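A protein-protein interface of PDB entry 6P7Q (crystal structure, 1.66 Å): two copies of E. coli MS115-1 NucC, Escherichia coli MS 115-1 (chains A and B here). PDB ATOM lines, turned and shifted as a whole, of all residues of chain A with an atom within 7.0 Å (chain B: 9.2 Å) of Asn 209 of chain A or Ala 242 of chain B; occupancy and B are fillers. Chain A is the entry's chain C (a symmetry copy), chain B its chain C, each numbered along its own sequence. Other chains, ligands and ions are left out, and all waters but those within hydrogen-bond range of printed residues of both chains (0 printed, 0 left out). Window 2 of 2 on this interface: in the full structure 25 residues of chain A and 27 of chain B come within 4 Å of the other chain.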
ATOM      1  N   SER A   9      -6.664 -17.998  27.234  1.00  0.00           N
ATOM      2  CA  SER A   9      -7.616 -17.127  27.903  1.00  0.00           C
ATOM      3  C   SER A   9      -7.396 -15.659  27.543  1.00  0.00           C
ATOM      4  O   SER A   9      -8.373 -14.911  27.341  1.00  0.00           O
ATOM      5  CB  SER A   9      -7.528 -17.306  29.431  1.00  0.00           C
ATOM      6  OG  SER A   9      -8.150 -18.514  29.793  1.00  0.00           O
ATOM      7  N   HIS A  16     -12.784  -9.840  23.236  1.00  0.00           N
ATOM      8  CA  HIS A  16     -13.936  -9.177  23.831  1.00  0.00           C
ATOM      9  C   HIS A  16     -13.660  -7.718  24.147  1.00  0.00           C
ATOM     10  O   HIS A  16     -14.499  -6.849  23.876  1.00  0.00           O
ATOM     11  CB  HIS A  16     -14.364  -9.884  25.126  1.00  0.00           C
ATOM     12  CG  HIS A  16     -15.314  -9.067  25.929  1.00  0.00           C
ATOM     13  ND1 HIS A  16     -16.653  -8.975  25.607  1.00  0.00           N
ATOM     14  CD2 HIS A  16     -15.094  -8.179  26.929  1.00  0.00           C
ATOM     15  CE1 HIS A  16     -17.225  -8.097  26.415  1.00  0.00           C
ATOM     16  NE2 HIS A  16     -16.304  -7.603  27.232  1.00  0.00           N
ATOM     17  N   HIS A 191     -22.131  -6.677  29.916  1.00  0.00           N
ATOM     18  CA  HIS A 191     -22.627  -7.481  31.038  1.00  0.00           C
ATOM     19  C   HIS A 191     -22.633  -8.995  30.866  1.00  0.00           C
ATOM     20  O   HIS A 191     -22.381  -9.725  31.836  1.00  0.00           O
ATOM     21  CB  HIS A 191     -24.071  -7.054  31.388  1.00  0.00           C
ATOM     22  CG  HIS A 191     -24.191  -5.624  31.818  1.00  0.00           C
ATOM     23  ND1 HIS A 191     -23.791  -5.200  33.065  1.00  0.00           N
ATOM     24  CD2 HIS A 191     -24.583  -4.515  31.147  1.00  0.00           C
ATOM     25  CE1 HIS A 191     -23.988  -3.896  33.159  1.00  0.00           C
ATOM     26  NE2 HIS A 191     -24.454  -3.455  32.004  1.00  0.00           N
ATOM     27  N   GLY A 192     -23.005  -9.498  29.693  1.00  0.00           N
ATOM     28  CA  GLY A 192     -23.090 -10.934  29.497  1.00  0.00           C
ATOM     29  C   GLY A 192     -23.810 -11.252  28.191  1.00  0.00           C
ATOM     30  O   GLY A 192     -23.842 -10.441  27.268  1.00  0.00           O
ATOM     31  N   HIS A 193     -24.405 -12.443  28.135  1.00  0.00           N
ATOM     32  CA  HIS A 193     -25.088 -12.861  26.924  1.00  0.00           C
ATOM     33  C   HIS A 193     -26.232 -13.767  27.329  1.00  0.00           C
ATOM     34  O   HIS A 193     -26.318 -14.202  28.466  1.00  0.00           O
ATOM     35  CB  HIS A 193     -24.102 -13.513  25.928  1.00  0.00           C
ATOM     36  CG  HIS A 193     -23.808 -14.961  26.192  1.00  0.00           C
ATOM     37  ND1 HIS A 193     -22.904 -15.374  27.142  1.00  0.00           N
ATOM     38  CD2 HIS A 193     -24.251 -16.085  25.584  1.00  0.00           C
ATOM     39  CE1 HIS A 193     -22.832 -16.695  27.144  1.00  0.00           C
ATOM     40  NE2 HIS A 193     -23.630 -17.150  26.192  1.00  0.00           N
ATOM     41  N   GLU A 206     -25.991 -15.617  30.948  1.00  0.00           N
ATOM     42  CA  GLU A 206     -24.636 -15.883  31.415  1.00  0.00           C
ATOM     43  C   GLU A 206     -23.922 -14.548  31.602  1.00  0.00           C
ATOM     44  O   GLU A 206     -23.800 -13.756  30.651  1.00  0.00           O
ATOM     45  CB  GLU A 206     -23.878 -16.776  30.440  1.00  0.00           C
ATOM     46  CG  GLU A 206     -24.432 -18.182  30.347  1.00  0.00           C
ATOM     47  CD  GLU A 206     -23.374 -19.197  29.962  1.00  0.00           C
ATOM     48  OE1 GLU A 206     -22.343 -18.794  29.375  1.00  0.00           O
ATOM     49  OE2 GLU A 206     -23.573 -20.398  30.250  1.00  0.00           O
ATOM     50  N   HIS A 207     -23.439 -14.309  32.811  1.00  0.00           N
ATOM     51  CA  HIS A 207     -22.860 -13.024  33.169  1.00  0.00           C
ATOM     52  C   HIS A 207     -21.353 -13.016  33.002  1.00  0.00           C
ATOM     53  O   HIS A 207     -20.672 -13.987  33.343  1.00  0.00           O
ATOM     54  CB  HIS A 207     -23.220 -12.672  34.623  1.00  0.00           C
ATOM     55  CG  HIS A 207     -24.694 -12.617  34.859  1.00  0.00           C
ATOM     56  ND1 HIS A 207     -25.470 -13.750  34.993  1.00  0.00           N
ATOM     57  CD2 HIS A 207     -25.540 -11.565  34.938  1.00  0.00           C
ATOM     58  CE1 HIS A 207     -26.730 -13.397  35.164  1.00  0.00           C
ATOM     59  NE2 HIS A 207     -26.799 -12.077  35.134  1.00  0.00           N
ATOM     60  N   GLY A 208     -20.836 -11.911  32.474  1.00  0.00           N
ATOM     61  CA  GLY A 208     -19.415 -11.705  32.314  1.00  0.00           C
ATOM     62  C   GLY A 208     -18.751 -12.809  31.523  1.00  0.00           C
ATOM     63  O   GLY A 208     -19.317 -13.361  30.567  1.00  0.00           O
ATOM     64  N   ASN A 209     -17.512 -13.117  31.908  1.00  0.00           N
ATOM     65  CA  ASN A 209     -16.714 -14.160  31.233  1.00  0.00           C
ATOM     66  C   ASN A 209     -16.666 -13.925  29.718  1.00  0.00           C
ATOM     67  O   ASN A 209     -17.039 -14.790  28.909  1.00  0.00           O
ATOM     68  CB  ASN A 209     -17.263 -15.555  31.547  1.00  0.00           C
ATOM     69  CG  ASN A 209     -17.113 -15.916  33.029  1.00  0.00           C
ATOM     70  OD1 ASN A 209     -16.126 -15.551  33.664  1.00  0.00           O
ATOM     71  ND2 ASN A 209     -18.105 -16.601  33.578  1.00  0.00           N
ATOM     72  N   LYS A 210     -16.193 -12.682  29.351  1.00  0.00           N
ATOM     73  CA  LYS A 210     -15.935 -12.301  27.972  1.00  0.00           C
ATOM     74  C   LYS A 210     -17.199 -12.377  27.103  1.00  0.00           C
ATOM     75  O   LYS A 210     -17.262 -13.162  26.151  1.00  0.00           O
ATOM     76  CB  LYS A 210     -14.802 -13.190  27.420  1.00  0.00           C
ATOM     77  CG  LYS A 210     -13.588 -13.261  28.362  1.00  0.00           C
ATOM     78  CD  LYS A 210     -12.567 -14.280  27.882  1.00  0.00           C
ATOM     79  CE  LYS A 210     -11.760 -14.895  29.031  1.00  0.00           C
ATOM     80  NZ  LYS A 210     -11.493 -13.938  30.108  1.00  0.00           N
ATOM     81  N   PRO A 211     -18.185 -11.534  27.381  1.00  0.00           N
ATOM     82  CA  PRO A 211     -19.504 -11.673  26.730  1.00  0.00           C
ATOM     83  C   PRO A 211     -19.499 -11.786  25.209  1.00  0.00           C
ATOM     84  O   PRO A 211     -20.199 -12.647  24.672  1.00  0.00           O
ATOM     85  CB  PRO A 211     -20.248 -10.400  27.219  1.00  0.00           C
ATOM     86  CG  PRO A 211     -19.715 -10.175  28.557  1.00  0.00           C
ATOM     87  CD  PRO A 211     -18.220 -10.568  28.510  1.00  0.00           C
ATOM     88  N   ALA A 212     -18.789 -10.917  24.497  1.00  0.00           N
ATOM     89  CA  ALA A 212     -18.827 -10.958  23.045  1.00  0.00           C
ATOM     90  C   ALA A 212     -18.186 -12.243  22.514  1.00  0.00           C
ATOM     91  O   ALA A 212     -18.679 -12.829  21.539  1.00  0.00           O
ATOM     92  CB  ALA A 212     -18.130  -9.719  22.458  1.00  0.00           C
ATOM     93  N   THR A 213     -17.109 -12.713  23.159  1.00  0.00           N
ATOM     94  CA  THR A 213     -16.494 -13.959  22.744  1.00  0.00           C
ATOM     95  C   THR A 213     -17.429 -15.141  23.022  1.00  0.00           C
ATOM     96  O   THR A 213     -17.534 -16.048  22.208  1.00  0.00           O
ATOM     97  CB  THR A 213     -15.160 -14.148  23.447  1.00  0.00           C
ATOM     98  OG1 THR A 213     -14.410 -12.913  23.341  1.00  0.00           O
ATOM     99  CG2 THR A 213     -14.386 -15.299  22.742  1.00  0.00           C
ATOM    100  N   ALA A 214     -18.113 -15.142  24.161  1.00  0.00           N
ATOM    101  CA  ALA A 214     -19.017 -16.239  24.484  1.00  0.00           C
ATOM    102  C   ALA A 214     -20.184 -16.269  23.503  1.00  0.00           C
ATOM    103  O   ALA A 214     -20.614 -17.337  23.044  1.00  0.00           O
ATOM    104  CB  ALA A 214     -19.511 -16.091  25.929  1.00  0.00           C
ATOM    105  N   PHE A 215     -20.703 -15.101  23.161  1.00  0.00           N
ATOM    106  CA  PHE A 215     -21.761 -15.028  22.156  1.00  0.00           C
ATOM    107  C   PHE A 215     -21.273 -15.563  20.809  1.00  0.00           C
ATOM    108  O   PHE A 215     -21.974 -16.356  20.155  1.00  0.00           O
ATOM    109  CB  PHE A 215     -22.280 -13.596  22.009  1.00  0.00           C
ATOM    110  CG  PHE A 215     -23.036 -13.376  20.712  1.00  0.00           C
ATOM    111  CD1 PHE A 215     -24.351 -13.753  20.614  1.00  0.00           C
ATOM    112  CD2 PHE A 215     -22.436 -12.827  19.632  1.00  0.00           C
ATOM    113  CE1 PHE A 215     -25.019 -13.590  19.409  1.00  0.00           C
ATOM    114  CE2 PHE A 215     -23.118 -12.651  18.404  1.00  0.00           C
ATOM    115  CZ  PHE A 215     -24.406 -13.046  18.332  1.00  0.00           C
ATOM    116  N   TYR B 237     -13.060 -24.869  23.156  1.00  0.00           N
ATOM    117  CA  TYR B 237     -12.315 -23.647  23.386  1.00  0.00           C
ATOM    118  C   TYR B 237     -13.010 -22.745  24.404  1.00  0.00           C
ATOM    119  O   TYR B 237     -12.340 -22.015  25.134  1.00  0.00           O
ATOM    120  CB  TYR B 237     -12.110 -22.895  22.051  1.00  0.00           C
ATOM    121  CG  TYR B 237     -11.104 -23.589  21.151  1.00  0.00           C
ATOM    122  CD1 TYR B 237     -11.497 -24.618  20.288  1.00  0.00           C
ATOM    123  CD2 TYR B 237      -9.785 -23.258  21.196  1.00  0.00           C
ATOM    124  CE1 TYR B 237     -10.569 -25.264  19.479  1.00  0.00           C
ATOM    125  CE2 TYR B 237      -8.835 -23.874  20.404  1.00  0.00           C
ATOM    126  CZ  TYR B 237      -9.231 -24.870  19.535  1.00  0.00           C
ATOM    127  OH  TYR B 237      -8.287 -25.467  18.829  1.00  0.00           O
ATOM    128  N   GLY B 238     -14.334 -22.775  24.464  1.00  0.00           N
ATOM    129  CA  GLY B 238     -15.088 -21.910  25.356  1.00  0.00           C
ATOM    130  C   GLY B 238     -14.921 -22.201  26.828  1.00  0.00           C
ATOM    131  O   GLY B 238     -15.340 -21.385  27.658  1.00  0.00           O
ATOM    132  N   LYS B 239     -14.338 -23.342  27.182  1.00  0.00           N
ATOM    133  CA  LYS B 239     -14.017 -23.587  28.572  1.00  0.00           C
ATOM    134  C   LYS B 239     -13.041 -22.557  29.113  1.00  0.00           C
ATOM    135  O   LYS B 239     -13.017 -22.321  30.324  1.00  0.00           O
ATOM    136  CB  LYS B 239     -13.468 -25.002  28.718  1.00  0.00           C
ATOM    137  CG  LYS B 239     -14.484 -26.066  28.317  1.00  0.00           C
ATOM    138  CD  LYS B 239     -13.802 -27.428  28.192  1.00  0.00           C
ATOM    139  CE  LYS B 239     -14.821 -28.565  28.165  1.00  0.00           C
ATOM    140  NZ  LYS B 239     -14.127 -29.873  27.964  1.00  0.00           N
ATOM    141  N   TRP B 240     -12.272 -21.898  28.244  1.00  0.00           N
ATOM    142  CA  TRP B 240     -11.299 -20.903  28.686  1.00  0.00           C
ATOM    143  C   TRP B 240     -11.884 -19.507  28.821  1.00  0.00           C
ATOM    144  O   TRP B 240     -11.157 -18.571  29.170  1.00  0.00           O
ATOM    145  CB  TRP B 240     -10.111 -20.861  27.713  1.00  0.00           C
ATOM    146  CG  TRP B 240      -9.404 -22.153  27.650  1.00  0.00           C
ATOM    147  CD1 TRP B 240      -9.684 -23.204  26.817  1.00  0.00           C
ATOM    148  CD2 TRP B 240      -8.320 -22.559  28.458  1.00  0.00           C
ATOM    149  NE1 TRP B 240      -8.823 -24.235  27.060  1.00  0.00           N
ATOM    150  CE2 TRP B 240      -7.980 -23.875  28.075  1.00  0.00           C
ATOM    151  CE3 TRP B 240      -7.607 -21.952  29.495  1.00  0.00           C
ATOM    152  CZ2 TRP B 240      -6.934 -24.586  28.674  1.00  0.00           C
ATOM    153  CZ3 TRP B 240      -6.572 -22.664  30.094  1.00  0.00           C
ATOM    154  CH2 TRP B 240      -6.253 -23.969  29.684  1.00  0.00           C
ATOM    155  N   LEU B 241     -13.181 -19.330  28.567  1.00  0.00           N
ATOM    156  CA  LEU B 241     -13.801 -18.031  28.795  1.00  0.00           C
ATOM    157  C   LEU B 241     -13.910 -17.714  30.285  1.00  0.00           C
ATOM    158  O   LEU B 241     -13.881 -16.544  30.667  1.00  0.00           O
ATOM    159  CB  LEU B 241     -15.168 -18.001  28.166  1.00  0.00           C
ATOM    160  CG  LEU B 241     -15.158 -18.222  26.654  1.00  0.00           C
ATOM    161  CD1 LEU B 241     -16.596 -18.398  26.172  1.00  0.00           C
ATOM    162  CD2 LEU B 241     -14.481 -17.086  25.969  1.00  0.00           C
ATOM    163  N   ALA B 242     -14.051 -18.725  31.130  1.00  0.00           N
ATOM    164  CA  ALA B 242     -14.204 -18.501  32.574  1.00  0.00           C
ATOM    165  C   ALA B 242     -12.858 -18.604  33.278  1.00  0.00           C
ATOM    166  O   ALA B 242     -12.014 -17.706  33.159  1.00  0.00           O
ATOM    167  CB  ALA B 242     -15.179 -19.503  33.160  1.00  0.00           C
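The backbone carbonyl oxygen of Trp 240 of chain B sits at hydrogen-bond distance from the side-chain hydroxyl of Ser 9 of chain A (3.1 Å).
N of His 16 of chain A lies within hydrogen-bond range of OG1 of Thr 213 of chain A (3.5 Å).
Among the printed residues, pairs that only touch across the chains: Lys 210 of chain A with Leu 241 of chain B (3.1 Å), Asn 209 of chain A with Leu 241 of chain B (3.6 Å), Ala 214 of chain A with Leu 241 of chain B (3.7 Å), Asn 209 of chain A with Ala 242 of chain B (3.7 Å), Thr 213 of chain A with Leu 241 of chain B (3.7 Å) and Lys 210 of chain A with Trp 240 of chain B (3.7 Å).
Of chain B, only Leu 241 and Ala 242 come within 4 Å of Asn 209 of chain A.
Of the printed residues of chain A, Trp 240 of chain B touches Ser 9 (3.1 Å) and Lys 210 (3.7 Å).
Of the printed residues of chain B, Thr 213 of chain A touches Leu 241.
Of the printed residues of chain B, Ala 214 of chain A touches Leu 241 (3.7 Å).
Gly 192 of chain A touches none of the printed residues of chain B.
The nearest residue of chain A that does not touch Ala 242 of chain B is Lys 210 of chain A (4.9 Å).
Hydrophobic or aromatic side chains of chain B that line the printed part of chain A: Trp 240 and Leu 241.
Along chain A the printed residues that touch a printed residue of chain B span positions 9 to 214.
Among the printed residues, 7 pairs touch across the chains.
Among the printed residues, no Asp or Glu carboxylate lies within 4 Å of a Lys or Arg side-chain nitrogen of the other chain.
No position is printed for both chains.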
